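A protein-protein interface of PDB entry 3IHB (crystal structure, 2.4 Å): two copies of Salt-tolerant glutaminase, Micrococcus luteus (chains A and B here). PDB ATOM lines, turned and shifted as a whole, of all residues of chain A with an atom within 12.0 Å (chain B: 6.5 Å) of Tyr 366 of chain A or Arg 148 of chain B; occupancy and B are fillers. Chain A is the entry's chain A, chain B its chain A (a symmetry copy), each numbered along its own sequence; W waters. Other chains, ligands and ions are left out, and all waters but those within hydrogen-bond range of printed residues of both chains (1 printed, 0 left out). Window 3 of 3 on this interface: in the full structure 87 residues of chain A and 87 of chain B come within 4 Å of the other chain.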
ATOM      1  N   GLY A 358      15.414  -1.728   4.712  1.00  0.00           N
ATOM      2  CA  GLY A 358      15.603  -1.674   6.147  1.00  0.00           C
ATOM      3  C   GLY A 358      17.062  -1.387   6.433  1.00  0.00           C
ATOM      4  O   GLY A 358      17.844  -2.309   6.672  1.00  0.00           O
ATOM      5  N   THR A 359      17.426  -0.104   6.391  1.00  0.00           N
ATOM      6  CA  THR A 359      18.795   0.350   6.639  1.00  0.00           C
ATOM      7  C   THR A 359      19.509  -0.603   7.581  1.00  0.00           C
ATOM      8  O   THR A 359      20.656  -0.982   7.358  1.00  0.00           O
ATOM      9  CB  THR A 359      18.819   1.754   7.297  1.00  0.00           C
ATOM     10  OG1 THR A 359      17.929   2.635   6.601  1.00  0.00           O
ATOM     11  CG2 THR A 359      20.232   2.335   7.262  1.00  0.00           C
ATOM     12  N   GLY A 360      18.804  -0.995   8.635  1.00  0.00           N
ATOM     13  CA  GLY A 360      19.377  -1.885   9.621  1.00  0.00           C
ATOM     14  C   GLY A 360      19.816  -1.030  10.786  1.00  0.00           C
ATOM     15  O   GLY A 360      19.749  -1.450  11.941  1.00  0.00           O
ATOM     16  N   TRP A 361      20.250   0.189  10.475  1.00  0.00           N
ATOM     17  CA  TRP A 361      20.707   1.127  11.491  1.00  0.00           C
ATOM     18  C   TRP A 361      20.039   2.502  11.384  1.00  0.00           C
ATOM     19  O   TRP A 361      19.676   2.952  10.294  1.00  0.00           O
ATOM     20  CB  TRP A 361      22.232   1.286  11.411  1.00  0.00           C
ATOM     21  CG  TRP A 361      22.739   1.717  10.063  1.00  0.00           C
ATOM     22  CD1 TRP A 361      22.946   0.927   8.970  1.00  0.00           C
ATOM     23  CD2 TRP A 361      23.091   3.048   9.668  1.00  0.00           C
ATOM     24  NE1 TRP A 361      23.408   1.683   7.918  1.00  0.00           N
ATOM     25  CE2 TRP A 361      23.504   2.991   8.319  1.00  0.00           C
ATOM     26  CE3 TRP A 361      23.097   4.287  10.323  1.00  0.00           C
ATOM     27  CZ2 TRP A 361      23.920   4.122   7.610  1.00  0.00           C
ATOM     28  CZ3 TRP A 361      23.511   5.413   9.621  1.00  0.00           C
ATOM     29  CH2 TRP A 361      23.916   5.323   8.279  1.00  0.00           C
ATOM     30  N   ASP A 362      19.890   3.159  12.532  1.00  0.00           N
ATOM     31  CA  ASP A 362      19.275   4.482  12.616  1.00  0.00           C
ATOM     32  C   ASP A 362      20.272   5.572  12.230  1.00  0.00           C
ATOM     33  O   ASP A 362      21.186   5.884  12.995  1.00  0.00           O
ATOM     34  CB  ASP A 362      18.784   4.734  14.044  1.00  0.00           C
ATOM     35  CG  ASP A 362      18.082   6.070  14.198  1.00  0.00           C
ATOM     36  OD1 ASP A 362      18.215   6.933  13.301  1.00  0.00           O
ATOM     37  OD2 ASP A 362      17.402   6.259  15.230  1.00  0.00           O
ATOM     38  N   ALA A 363      20.082   6.153  11.050  1.00  0.00           N
ATOM     39  CA  ALA A 363      20.954   7.211  10.550  1.00  0.00           C
ATOM     40  C   ALA A 363      21.119   8.345  11.555  1.00  0.00           C
ATOM     41  O   ALA A 363      22.180   8.962  11.637  1.00  0.00           O
ATOM     42  CB  ALA A 363      20.404   7.753   9.244  1.00  0.00           C
ATOM     43  N   ALA A 364      20.064   8.619  12.313  1.00  0.00           N
ATOM     44  CA  ALA A 364      20.096   9.678  13.313  1.00  0.00           C
ATOM     45  C   ALA A 364      21.100   9.350  14.411  1.00  0.00           C
ATOM     46  O   ALA A 364      21.797  10.232  14.922  1.00  0.00           O
ATOM     47  CB  ALA A 364      18.713   9.862  13.909  1.00  0.00           C
ATOM     48  N   VAL A 365      21.172   8.073  14.769  1.00  0.00           N
ATOM     49  CA  VAL A 365      22.082   7.622  15.814  1.00  0.00           C
ATOM     50  C   VAL A 365      23.519   7.500  15.320  1.00  0.00           C
ATOM     51  O   VAL A 365      24.460   7.795  16.055  1.00  0.00           O
ATOM     52  CB  VAL A 365      21.626   6.263  16.390  1.00  0.00           C
ATOM     53  CG1 VAL A 365      22.616   5.770  17.432  1.00  0.00           C
ATOM     54  CG2 VAL A 365      20.246   6.403  17.001  1.00  0.00           C
ATOM     55  N   TYR A 366      23.694   7.074  14.074  1.00  0.00           N
ATOM     56  CA  TYR A 366      25.035   6.919  13.525  1.00  0.00           C
ATOM     57  C   TYR A 366      25.338   7.915  12.416  1.00  0.00           C
ATOM     58  O   TYR A 366      25.415   7.548  11.245  1.00  0.00           O
ATOM     59  CB  TYR A 366      25.241   5.502  12.971  1.00  0.00           C
ATOM     60  CG  TYR A 366      24.966   4.374  13.941  1.00  0.00           C
ATOM     61  CD1 TYR A 366      23.678   3.875  14.113  1.00  0.00           C
ATOM     62  CD2 TYR A 366      26.002   3.785  14.665  1.00  0.00           C
ATOM     63  CE1 TYR A 366      23.428   2.808  14.982  1.00  0.00           C
ATOM     64  CE2 TYR A 366      25.765   2.718  15.536  1.00  0.00           C
ATOM     65  CZ  TYR A 366      24.478   2.234  15.685  1.00  0.00           C
ATOM     66  OH  TYR A 366      24.245   1.162  16.514  1.00  0.00           O
ATOM     67  N   PRO A 367      25.526   9.195  12.763  1.00  0.00           N
ATOM     68  CA  PRO A 367      25.822  10.154  11.696  1.00  0.00           C
ATOM     69  C   PRO A 367      27.060   9.763  10.884  1.00  0.00           C
ATOM     70  O   PRO A 367      27.108   9.960   9.669  1.00  0.00           O
ATOM     71  CB  PRO A 367      25.995  11.473  12.457  1.00  0.00           C
ATOM     72  CG  PRO A 367      26.433  11.036  13.832  1.00  0.00           C
ATOM     73  CD  PRO A 367      25.548   9.846  14.085  1.00  0.00           C
ATOM     74  N   ARG A 368      28.052   9.191  11.557  1.00  0.00           N
ATOM     75  CA  ARG A 368      29.284   8.781  10.895  1.00  0.00           C
ATOM     76  C   ARG A 368      29.005   7.775   9.785  1.00  0.00           C
ATOM     77  O   ARG A 368      29.513   7.902   8.671  1.00  0.00           O
ATOM     78  CB  ARG A 368      30.250   8.153  11.905  1.00  0.00           C
ATOM     79  CG  ARG A 368      30.683   9.061  13.055  1.00  0.00           C
ATOM     80  CD  ARG A 368      31.581  10.210  12.599  1.00  0.00           C
ATOM     81  NE  ARG A 368      30.834  11.299  11.977  1.00  0.00           N
ATOM     82  CZ  ARG A 368      29.883  12.002  12.588  1.00  0.00           C
ATOM     83  NH1 ARG A 368      29.555  11.732  13.846  1.00  0.00           N
ATOM     84  NH2 ARG A 368      29.257  12.977  11.940  1.00  0.00           N
ATOM     85  N   TRP A 369      28.194   6.774  10.094  1.00  0.00           N
ATOM     86  CA  TRP A 369      27.862   5.739   9.124  1.00  0.00           C
ATOM     87  C   TRP A 369      27.165   6.275   7.882  1.00  0.00           C
ATOM     88  O   TRP A 369      27.427   5.814   6.768  1.00  0.00           O
ATOM     89  CB  TRP A 369      26.990   4.669   9.781  1.00  0.00           C
ATOM     90  CG  TRP A 369      27.688   3.917  10.870  1.00  0.00           C
ATOM     91  CD1 TRP A 369      28.873   4.245  11.468  1.00  0.00           C
ATOM     92  CD2 TRP A 369      27.227   2.732  11.519  1.00  0.00           C
ATOM     93  NE1 TRP A 369      29.176   3.338  12.451  1.00  0.00           N
ATOM     94  CE2 TRP A 369      28.180   2.393  12.504  1.00  0.00           C
ATOM     95  CE3 TRP A 369      26.094   1.918  11.367  1.00  0.00           C
ATOM     96  CZ2 TRP A 369      28.040   1.279  13.335  1.00  0.00           C
ATOM     97  CZ3 TRP A 369      25.953   0.811  12.195  1.00  0.00           C
ATOM     98  CH2 TRP A 369      26.922   0.501  13.166  1.00  0.00           C
ATOM     99  N   GLN A 370      26.275   7.245   8.072  1.00  0.00           N
ATOM    100  CA  GLN A 370      25.551   7.818   6.947  1.00  0.00           C
ATOM    101  C   GLN A 370      26.498   8.592   6.046  1.00  0.00           C
ATOM    102  O   GLN A 370      26.405   8.512   4.821  1.00  0.00           O
ATOM    103  CB  GLN A 370      24.425   8.731   7.438  1.00  0.00           C
ATOM    104  CG  GLN A 370      23.668   9.407   6.312  1.00  0.00           C
ATOM    105  CD  GLN A 370      22.389  10.067   6.779  1.00  0.00           C
ATOM    106  OE1 GLN A 370      21.427   9.391   7.136  1.00  0.00           O
ATOM    107  NE2 GLN A 370      22.372  11.397   6.783  1.00  0.00           N
ATOM    108  N   GLU A 371      27.415   9.336   6.657  1.00  0.00           N
ATOM    109  CA  GLU A 371      28.378  10.111   5.893  1.00  0.00           C
ATOM    110  C   GLU A 371      29.205   9.163   5.045  1.00  0.00           C
ATOM    111  O   GLU A 371      29.326   9.342   3.834  1.00  0.00           O
ATOM    112  CB  GLU A 371      29.300  10.893   6.825  1.00  0.00           C
ATOM    113  CG  GLU A 371      28.563  11.794   7.790  1.00  0.00           C
ATOM    114  CD  GLU A 371      29.499  12.528   8.723  1.00  0.00           C
ATOM    115  OE1 GLU A 371      30.306  11.859   9.401  1.00  0.00           O
ATOM    116  OE2 GLU A 371      29.425  13.773   8.782  1.00  0.00           O
ATOM    117  N   ALA A 372      29.765   8.146   5.691  1.00  0.00           N
ATOM    118  CA  ALA A 372      30.593   7.166   5.005  1.00  0.00           C
ATOM    119  C   ALA A 372      29.820   6.511   3.872  1.00  0.00           C
ATOM    120  O   ALA A 372      30.371   6.264   2.797  1.00  0.00           O
ATOM    121  CB  ALA A 372      31.076   6.108   5.992  1.00  0.00           C
ATOM    122  N   ALA A 373      28.544   6.232   4.119  1.00  0.00           N
ATOM    123  CA  ALA A 373      27.685   5.610   3.117  1.00  0.00           C
ATOM    124  C   ALA A 373      27.431   6.561   1.947  1.00  0.00           C
ATOM    125  O   ALA A 373      27.216   6.119   0.818  1.00  0.00           O
ATOM    126  CB  ALA A 373      26.358   5.196   3.749  1.00  0.00           C
ATOM    127  N   ALA A 374      27.456   7.863   2.222  1.00  0.00           N
ATOM    128  CA  ALA A 374      27.224   8.875   1.192  1.00  0.00           C
ATOM    129  C   ALA A 374      28.188   8.700   0.017  1.00  0.00           C
ATOM    130  O   ALA A 374      27.859   9.029  -1.121  1.00  0.00           O
ATOM    131  CB  ALA A 374      27.366  10.270   1.791  1.00  0.00           C
ATOM    132  N   ASP A 375      29.381   8.186   0.302  1.00  0.00           N
ATOM    133  CA  ASP A 375      30.381   7.948  -0.733  1.00  0.00           C
ATOM    134  C   ASP A 375      30.622   6.439  -0.812  1.00  0.00           C
ATOM    135  O   ASP A 375      31.566   5.916  -0.219  1.00  0.00           O
ATOM    136  CB  ASP A 375      31.686   8.664  -0.388  1.00  0.00           C
ATOM    137  CG  ASP A 375      32.706   8.574  -1.503  1.00  0.00           C
ATOM    138  OD1 ASP A 375      32.868   7.474  -2.069  1.00  0.00           O
ATOM    139  OD2 ASP A 375      33.348   9.600  -1.812  1.00  0.00           O
ATOM    140  N   LEU A 379      33.877   3.857   0.441  1.00  0.00           N
ATOM    141  CA  LEU A 379      33.658   2.853   1.470  1.00  0.00           C
ATOM    142  C   LEU A 379      33.867   1.454   0.895  1.00  0.00           C
ATOM    143  O   LEU A 379      34.298   0.549   1.608  1.00  0.00           O
ATOM    144  CB  LEU A 379      32.241   2.987   2.053  1.00  0.00           C
ATOM    145  CG  LEU A 379      31.817   2.061   3.207  1.00  0.00           C
ATOM    146  CD1 LEU A 379      32.764   2.173   4.398  1.00  0.00           C
ATOM    147  CD2 LEU A 379      30.412   2.425   3.630  1.00  0.00           C
ATOM    148  N   GLU B  59      18.790  -4.908  24.344  1.00  0.00           N
ATOM    149  CA  GLU B  59      20.071  -4.803  25.031  1.00  0.00           C
ATOM    150  C   GLU B  59      20.215  -5.823  26.161  1.00  0.00           C
ATOM    151  O   GLU B  59      19.237  -6.196  26.811  1.00  0.00           O
ATOM    152  CB  GLU B  59      20.264  -3.399  25.607  1.00  0.00           C
ATOM    153  CG  GLU B  59      20.404  -2.289  24.581  1.00  0.00           C
ATOM    154  CD  GLU B  59      20.835  -0.975  25.226  1.00  0.00           C
ATOM    155  OE1 GLU B  59      20.449  -0.743  26.395  1.00  0.00           O
ATOM    156  OE2 GLU B  59      21.548  -0.177  24.573  1.00  0.00           O
ATOM    157  N   VAL B 139      35.181   0.591  28.233  1.00  0.00           N
ATOM    158  CA  VAL B 139      33.954   1.074  27.628  1.00  0.00           C
ATOM    159  C   VAL B 139      34.255   1.739  26.287  1.00  0.00           C
ATOM    160  O   VAL B 139      33.451   1.670  25.360  1.00  0.00           O
ATOM    161  CB  VAL B 139      33.246   2.088  28.553  1.00  0.00           C
ATOM    162  CG1 VAL B 139      31.897   2.486  27.964  1.00  0.00           C
ATOM    163  CG2 VAL B 139      33.056   1.481  29.932  1.00  0.00           C
ATOM    164  N   MET B 142      35.038  -0.991  23.282  1.00  0.00           N
ATOM    165  CA  MET B 142      33.799  -1.628  22.843  1.00  0.00           C
ATOM    166  C   MET B 142      32.927  -0.626  22.079  1.00  0.00           C
ATOM    167  O   MET B 142      32.348  -0.959  21.041  1.00  0.00           O
ATOM    168  CB  MET B 142      33.037  -2.201  24.046  1.00  0.00           C
ATOM    169  CG  MET B 142      33.650  -3.491  24.588  1.00  0.00           C
ATOM    170  SD  MET B 142      32.919  -4.107  26.118  1.00  0.00           S
ATOM    171  CE  MET B 142      31.664  -5.092  25.499  1.00  0.00           C
ATOM    172  N   SER B 143      32.861   0.604  22.593  1.00  0.00           N
ATOM    173  CA  SER B 143      32.083   1.679  21.984  1.00  0.00           C
ATOM    174  C   SER B 143      32.590   2.076  20.605  1.00  0.00           C
ATOM    175  O   SER B 143      31.804   2.353  19.700  1.00  0.00           O
ATOM    176  CB  SER B 143      32.095   2.910  22.886  1.00  0.00           C
ATOM    177  OG  SER B 143      31.365   2.670  24.078  1.00  0.00           O
ATOM    178  N   LEU B 144      33.905   2.109  20.442  1.00  0.00           N
ATOM    179  CA  LEU B 144      34.481   2.494  19.162  1.00  0.00           C
ATOM    180  C   LEU B 144      34.217   1.482  18.051  1.00  0.00           C
ATOM    181  O   LEU B 144      34.108   1.862  16.879  1.00  0.00           O
ATOM    182  CB  LEU B 144      35.986   2.736  19.317  1.00  0.00           C
ATOM    183  CG  LEU B 144      36.338   3.926  20.222  1.00  0.00           C
ATOM    184  CD1 LEU B 144      37.855   4.015  20.428  1.00  0.00           C
ATOM    185  CD2 LEU B 144      35.798   5.211  19.597  1.00  0.00           C
ATOM    186  N   LEU B 145      34.110   0.202  18.403  1.00  0.00           N
ATOM    187  CA  LEU B 145      33.858  -0.816  17.384  1.00  0.00           C
ATOM    188  C   LEU B 145      32.357  -0.947  17.136  1.00  0.00           C
ATOM    189  O   LEU B 145      31.923  -1.249  16.018  1.00  0.00           O
ATOM    190  CB  LEU B 145      34.445  -2.169  17.799  1.00  0.00           C
ATOM    191  CG  LEU B 145      35.942  -2.251  18.118  1.00  0.00           C
ATOM    192  CD1 LEU B 145      36.345  -3.708  18.212  1.00  0.00           C
ATOM    193  CD2 LEU B 145      36.757  -1.570  17.052  1.00  0.00           C
ATOM    194  N   ALA B 146      31.573  -0.709  18.185  1.00  0.00           N
ATOM    195  CA  ALA B 146      30.119  -0.784  18.099  1.00  0.00           C
ATOM    196  C   ALA B 146      29.593   0.429  17.339  1.00  0.00           C
ATOM    197  O   ALA B 146      28.452   0.430  16.857  1.00  0.00           O
ATOM    198  CB  ALA B 146      29.515  -0.823  19.490  1.00  0.00           C
ATOM    199  N   GLY B 147      30.432   1.462  17.242  1.00  0.00           N
ATOM    200  CA  GLY B 147      30.049   2.671  16.536  1.00  0.00           C
ATOM    201  C   GLY B 147      29.205   3.671  17.320  1.00  0.00           C
ATOM    202  O   GLY B 147      28.726   4.646  16.748  1.00  0.00           O
ATOM    203  N   ARG B 148      29.017   3.443  18.616  1.00  0.00           N
ATOM    204  CA  ARG B 148      28.228   4.351  19.435  1.00  0.00           C
ATOM    205  C   ARG B 148      28.633   4.238  20.903  1.00  0.00           C
ATOM    206  O   ARG B 148      29.122   3.198  21.337  1.00  0.00           O
ATOM    207  CB  ARG B 148      26.739   4.032  19.296  1.00  0.00           C
ATOM    208  CG  ARG B 148      26.325   2.730  19.965  1.00  0.00           C
ATOM    209  CD  ARG B 148      24.865   2.405  19.720  1.00  0.00           C
ATOM    210  NE  ARG B 148      24.498   1.129  20.323  1.00  0.00           N
ATOM    211  CZ  ARG B 148      23.991   0.981  21.543  1.00  0.00           C
ATOM    212  NH1 ARG B 148      23.703  -0.235  21.990  1.00  0.00           N
ATOM    213  NH2 ARG B 148      23.753   2.039  22.307  1.00  0.00           N
ATOM    214  N   ARG B 149      28.417   5.310  21.659  1.00  0.00           N
ATOM    215  CA  ARG B 149      28.746   5.339  23.075  1.00  0.00           C
ATOM    216  C   ARG B 149      27.880   4.346  23.853  1.00  0.00           C
ATOM    217  O   ARG B 149      26.658   4.481  23.901  1.00  0.00           O
ATOM    218  CB  ARG B 149      28.534   6.748  23.630  1.00  0.00           C
ATOM    219  CG  ARG B 149      28.872   6.881  25.107  1.00  0.00           C
ATOM    220  CD  ARG B 149      27.892   7.803  25.813  1.00  0.00           C
ATOM    221  NE  ARG B 149      28.004   7.716  27.267  1.00  0.00           N
ATOM    222  CZ  ARG B 149      27.049   8.103  28.109  1.00  0.00           C
ATOM    223  NH1 ARG B 149      25.912   8.603  27.641  1.00  0.00           N
ATOM    224  NH2 ARG B 149      27.230   7.991  29.420  1.00  0.00           N
ATOM    225  N   LEU B 150      28.524   3.348  24.457  1.00  0.00           N
ATOM    226  CA  LEU B 150      27.820   2.327  25.231  1.00  0.00           C
ATOM    227  C   LEU B 150      27.786   2.723  26.695  1.00  0.00           C
ATOM    228  O   LEU B 150      28.503   3.616  27.113  1.00  0.00           O
ATOM    229  CB  LEU B 150      28.519   0.968  25.097  1.00  0.00           C
ATOM    230  CG  LEU B 150      28.613   0.363  23.695  1.00  0.00           C
ATOM    231  CD1 LEU B 150      29.462  -0.905  23.730  1.00  0.00           C
ATOM    232  CD2 LEU B 150      27.213   0.066  23.183  1.00  0.00           C
ATOM    233  N   SER B 151      26.961   2.040  27.475  1.00  0.00           N
ATOM    234  CA  SER B 151      26.853   2.342  28.890  1.00  0.00           C
ATOM    235  C   SER B 151      26.883   1.081  29.734  1.00  0.00           C
ATOM    236  O   SER B 151      26.653  -0.017  29.230  1.00  0.00           O
ATOM    237  CB  SER B 151      25.555   3.108  29.166  1.00  0.00           C
ATOM    238  OG  SER B 151      25.542   4.352  28.489  1.00  0.00           O
ATOM    239  N   LEU B 198      26.189  -2.702  28.214  1.00  0.00           N
ATOM    240  CA  LEU B 198      25.012  -3.116  27.450  1.00  0.00           C
ATOM    241  C   LEU B 198      25.158  -3.047  25.931  1.00  0.00           C
ATOM    242  O   LEU B 198      25.585  -2.034  25.379  1.00  0.00           O
ATOM    243  CB  LEU B 198      23.816  -2.276  27.879  1.00  0.00           C
ATOM    244  CG  LEU B 198      23.411  -2.483  29.336  1.00  0.00           C
ATOM    245  CD1 LEU B 198      22.697  -1.246  29.853  1.00  0.00           C
ATOM    246  CD2 LEU B 198      22.543  -3.739  29.451  1.00  0.00           C
ATOM    247  N   VAL B 199      24.780  -4.133  25.263  1.00  0.00           N
ATOM    248  CA  VAL B 199      24.857  -4.226  23.807  1.00  0.00           C
ATOM    249  C   VAL B 199      23.652  -5.002  23.277  1.00  0.00           C
ATOM    250  O   VAL B 199      22.962  -5.699  24.026  1.00  0.00           O
ATOM    251  CB  VAL B 199      26.139  -4.982  23.351  1.00  0.00           C
ATOM    252  CG1 VAL B 199      27.387  -4.230  23.774  1.00  0.00           C
ATOM    253  CG2 VAL B 199      26.151  -6.388  23.956  1.00  0.00           C
ATOM    254  N   THR B 200      23.401  -4.876  21.984  1.00  0.00           N
ATOM    255  CA  THR B 200      22.307  -5.601  21.354  1.00  0.00           C
ATOM    256  C   THR B 200      22.919  -6.645  20.413  1.00  0.00           C
ATOM    257  O   THR B 200      24.123  -6.640  20.149  1.00  0.00           O
ATOM    258  CB  THR B 200      21.412  -4.675  20.501  1.00  0.00           C
ATOM    259  OG1 THR B 200      22.182  -4.143  19.418  1.00  0.00           O
ATOM    260  CG2 THR B 200      20.848  -3.533  21.343  1.00  0.00           C
ATOM    261  N   LYS B 202      22.809  -6.690  17.439  1.00  0.00           N
ATOM    262  CA  LYS B 202      23.387  -5.988  16.300  1.00  0.00           C
ATOM    263  C   LYS B 202      24.701  -5.283  16.609  1.00  0.00           C
ATOM    264  O   LYS B 202      25.537  -5.115  15.719  1.00  0.00           O
ATOM    265  CB  LYS B 202      22.349  -5.024  15.707  1.00  0.00           C
ATOM    266  CG  LYS B 202      21.084  -5.773  15.273  1.00  0.00           C
ATOM    267  CD  LYS B 202      20.254  -5.044  14.230  1.00  0.00           C
ATOM    268  CE  LYS B 202      19.426  -3.938  14.834  1.00  0.00           C
ATOM    269  NZ  LYS B 202      18.462  -3.404  13.830  1.00  0.00           N
ATOM    270  N   ASP B 203      24.895  -4.875  17.860  1.00  0.00           N
ATOM    271  CA  ASP B 203      26.150  -4.241  18.243  1.00  0.00           C
ATOM    272  C   ASP B 203      27.228  -5.321  18.076  1.00  0.00           C
ATOM    273  O   ASP B 203      28.241  -5.108  17.401  1.00  0.00           O
ATOM    274  CB  ASP B 203      26.118  -3.777  19.708  1.00  0.00           C
ATOM    275  CG  ASP B 203      25.096  -2.666  19.967  1.00  0.00           C
ATOM    276  OD1 ASP B 203      25.123  -1.636  19.254  1.00  0.00           O
ATOM    277  OD2 ASP B 203      24.275  -2.816  20.900  1.00  0.00           O
ATOM    278  N   VAL B 206      28.313  -6.148  14.518  1.00  0.00           N
ATOM    279  CA  VAL B 206      29.185  -5.108  13.982  1.00  0.00           C
ATOM    280  C   VAL B 206      30.557  -5.139  14.659  1.00  0.00           C
ATOM    281  O   VAL B 206      31.590  -4.996  14.001  1.00  0.00           O
ATOM    282  CB  VAL B 206      28.522  -3.694  14.140  1.00  0.00           C
ATOM    283  CG1 VAL B 206      29.418  -2.608  13.550  1.00  0.00           C
ATOM    284  CG2 VAL B 206      27.174  -3.678  13.427  1.00  0.00           C
HETATM  285  O   HOH W   1      26.102  -0.588  16.610  1.00  0.00           O
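O of Gly 360 of chain A is in hydrogen-bond range of NZ of Lys 202 of chain B (3.0 Å).
NH1 of Arg 148 of chain B is in salt-bridge range of OD2 of Asp 203 of chain B. N of Lys 202 of chain B lies close to OG1 of Thr 200 of chain B. The side-chain carboxylate of Glu 59 of chain B is in salt-bridge range of the guanidinium group of Arg 148 of chain B. The backbone NH of Arg 148 of chain B sits at hydrogen-bond distance from the backbone carbonyl oxygen of Ser 143 of chain B, at 3.2 Å.
Among the printed residues, merely in contact across the chains: Tyr 366 of chain A with Ala 146 of chain B, Tyr 366 of chain A with Gly 147 of chain B, Tyr 366 of chain A with Arg 148 of chain B and Trp 369 of chain A with Ala 146 of chain B.
Of the printed residues of chain B, Tyr 366 of chain A touches Ala 146, Gly 147 and Arg 148. Of chain A, only Tyr 366 (3.5 Å) comes within 4 Å of Arg 148 of chain B. No residue of chain A comes within 4 Å of Ser 143 of chain B. Ala 146 of chain B touches just these residues of chain A: Tyr 366 and Trp 369. Of the printed residues of chain A, Gly 147 of chain B touches Tyr 366 (3.5 Å). No residue of chain A comes within 4 Å of Leu 150 of chain B. No residue of chain A comes within 4 Å of Val 199 of chain B. Lys 202 of chain B touches just one residue of chain A: Gly 360. Printed residues of chain B within 4 Å of Gly 360 of chain A: Lys 202 (3.0 Å). Of the printed residues of chain B, Trp 369 of chain A touches Ala 146 (3.6 Å). The nearest printed residue of chain B that does not touch Tyr 366 of chain A is Asp 203 of chain B (4.01 Å).
Printed residues of chain B that touch a printed residue of chain A: Ala 146, Gly 147, Arg 148 and Lys 202. Hydrophobic or aromatic side chains of chain A within 4 Å of the printed part of chain B: Tyr 366 and Trp 369.
No position is printed for both chains. Of the 5 pairs that touch across the chains among the printed residues, none has its exchanged pair printed and touching as well.
Water W1 lies within hydrogen-bond range of the side-chain hydroxyl of Tyr 366 of chain A, the backbone carbonyl oxygen of Ala 146 of chain B and the side-chain carboxylate of Asp 203 of chain B.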
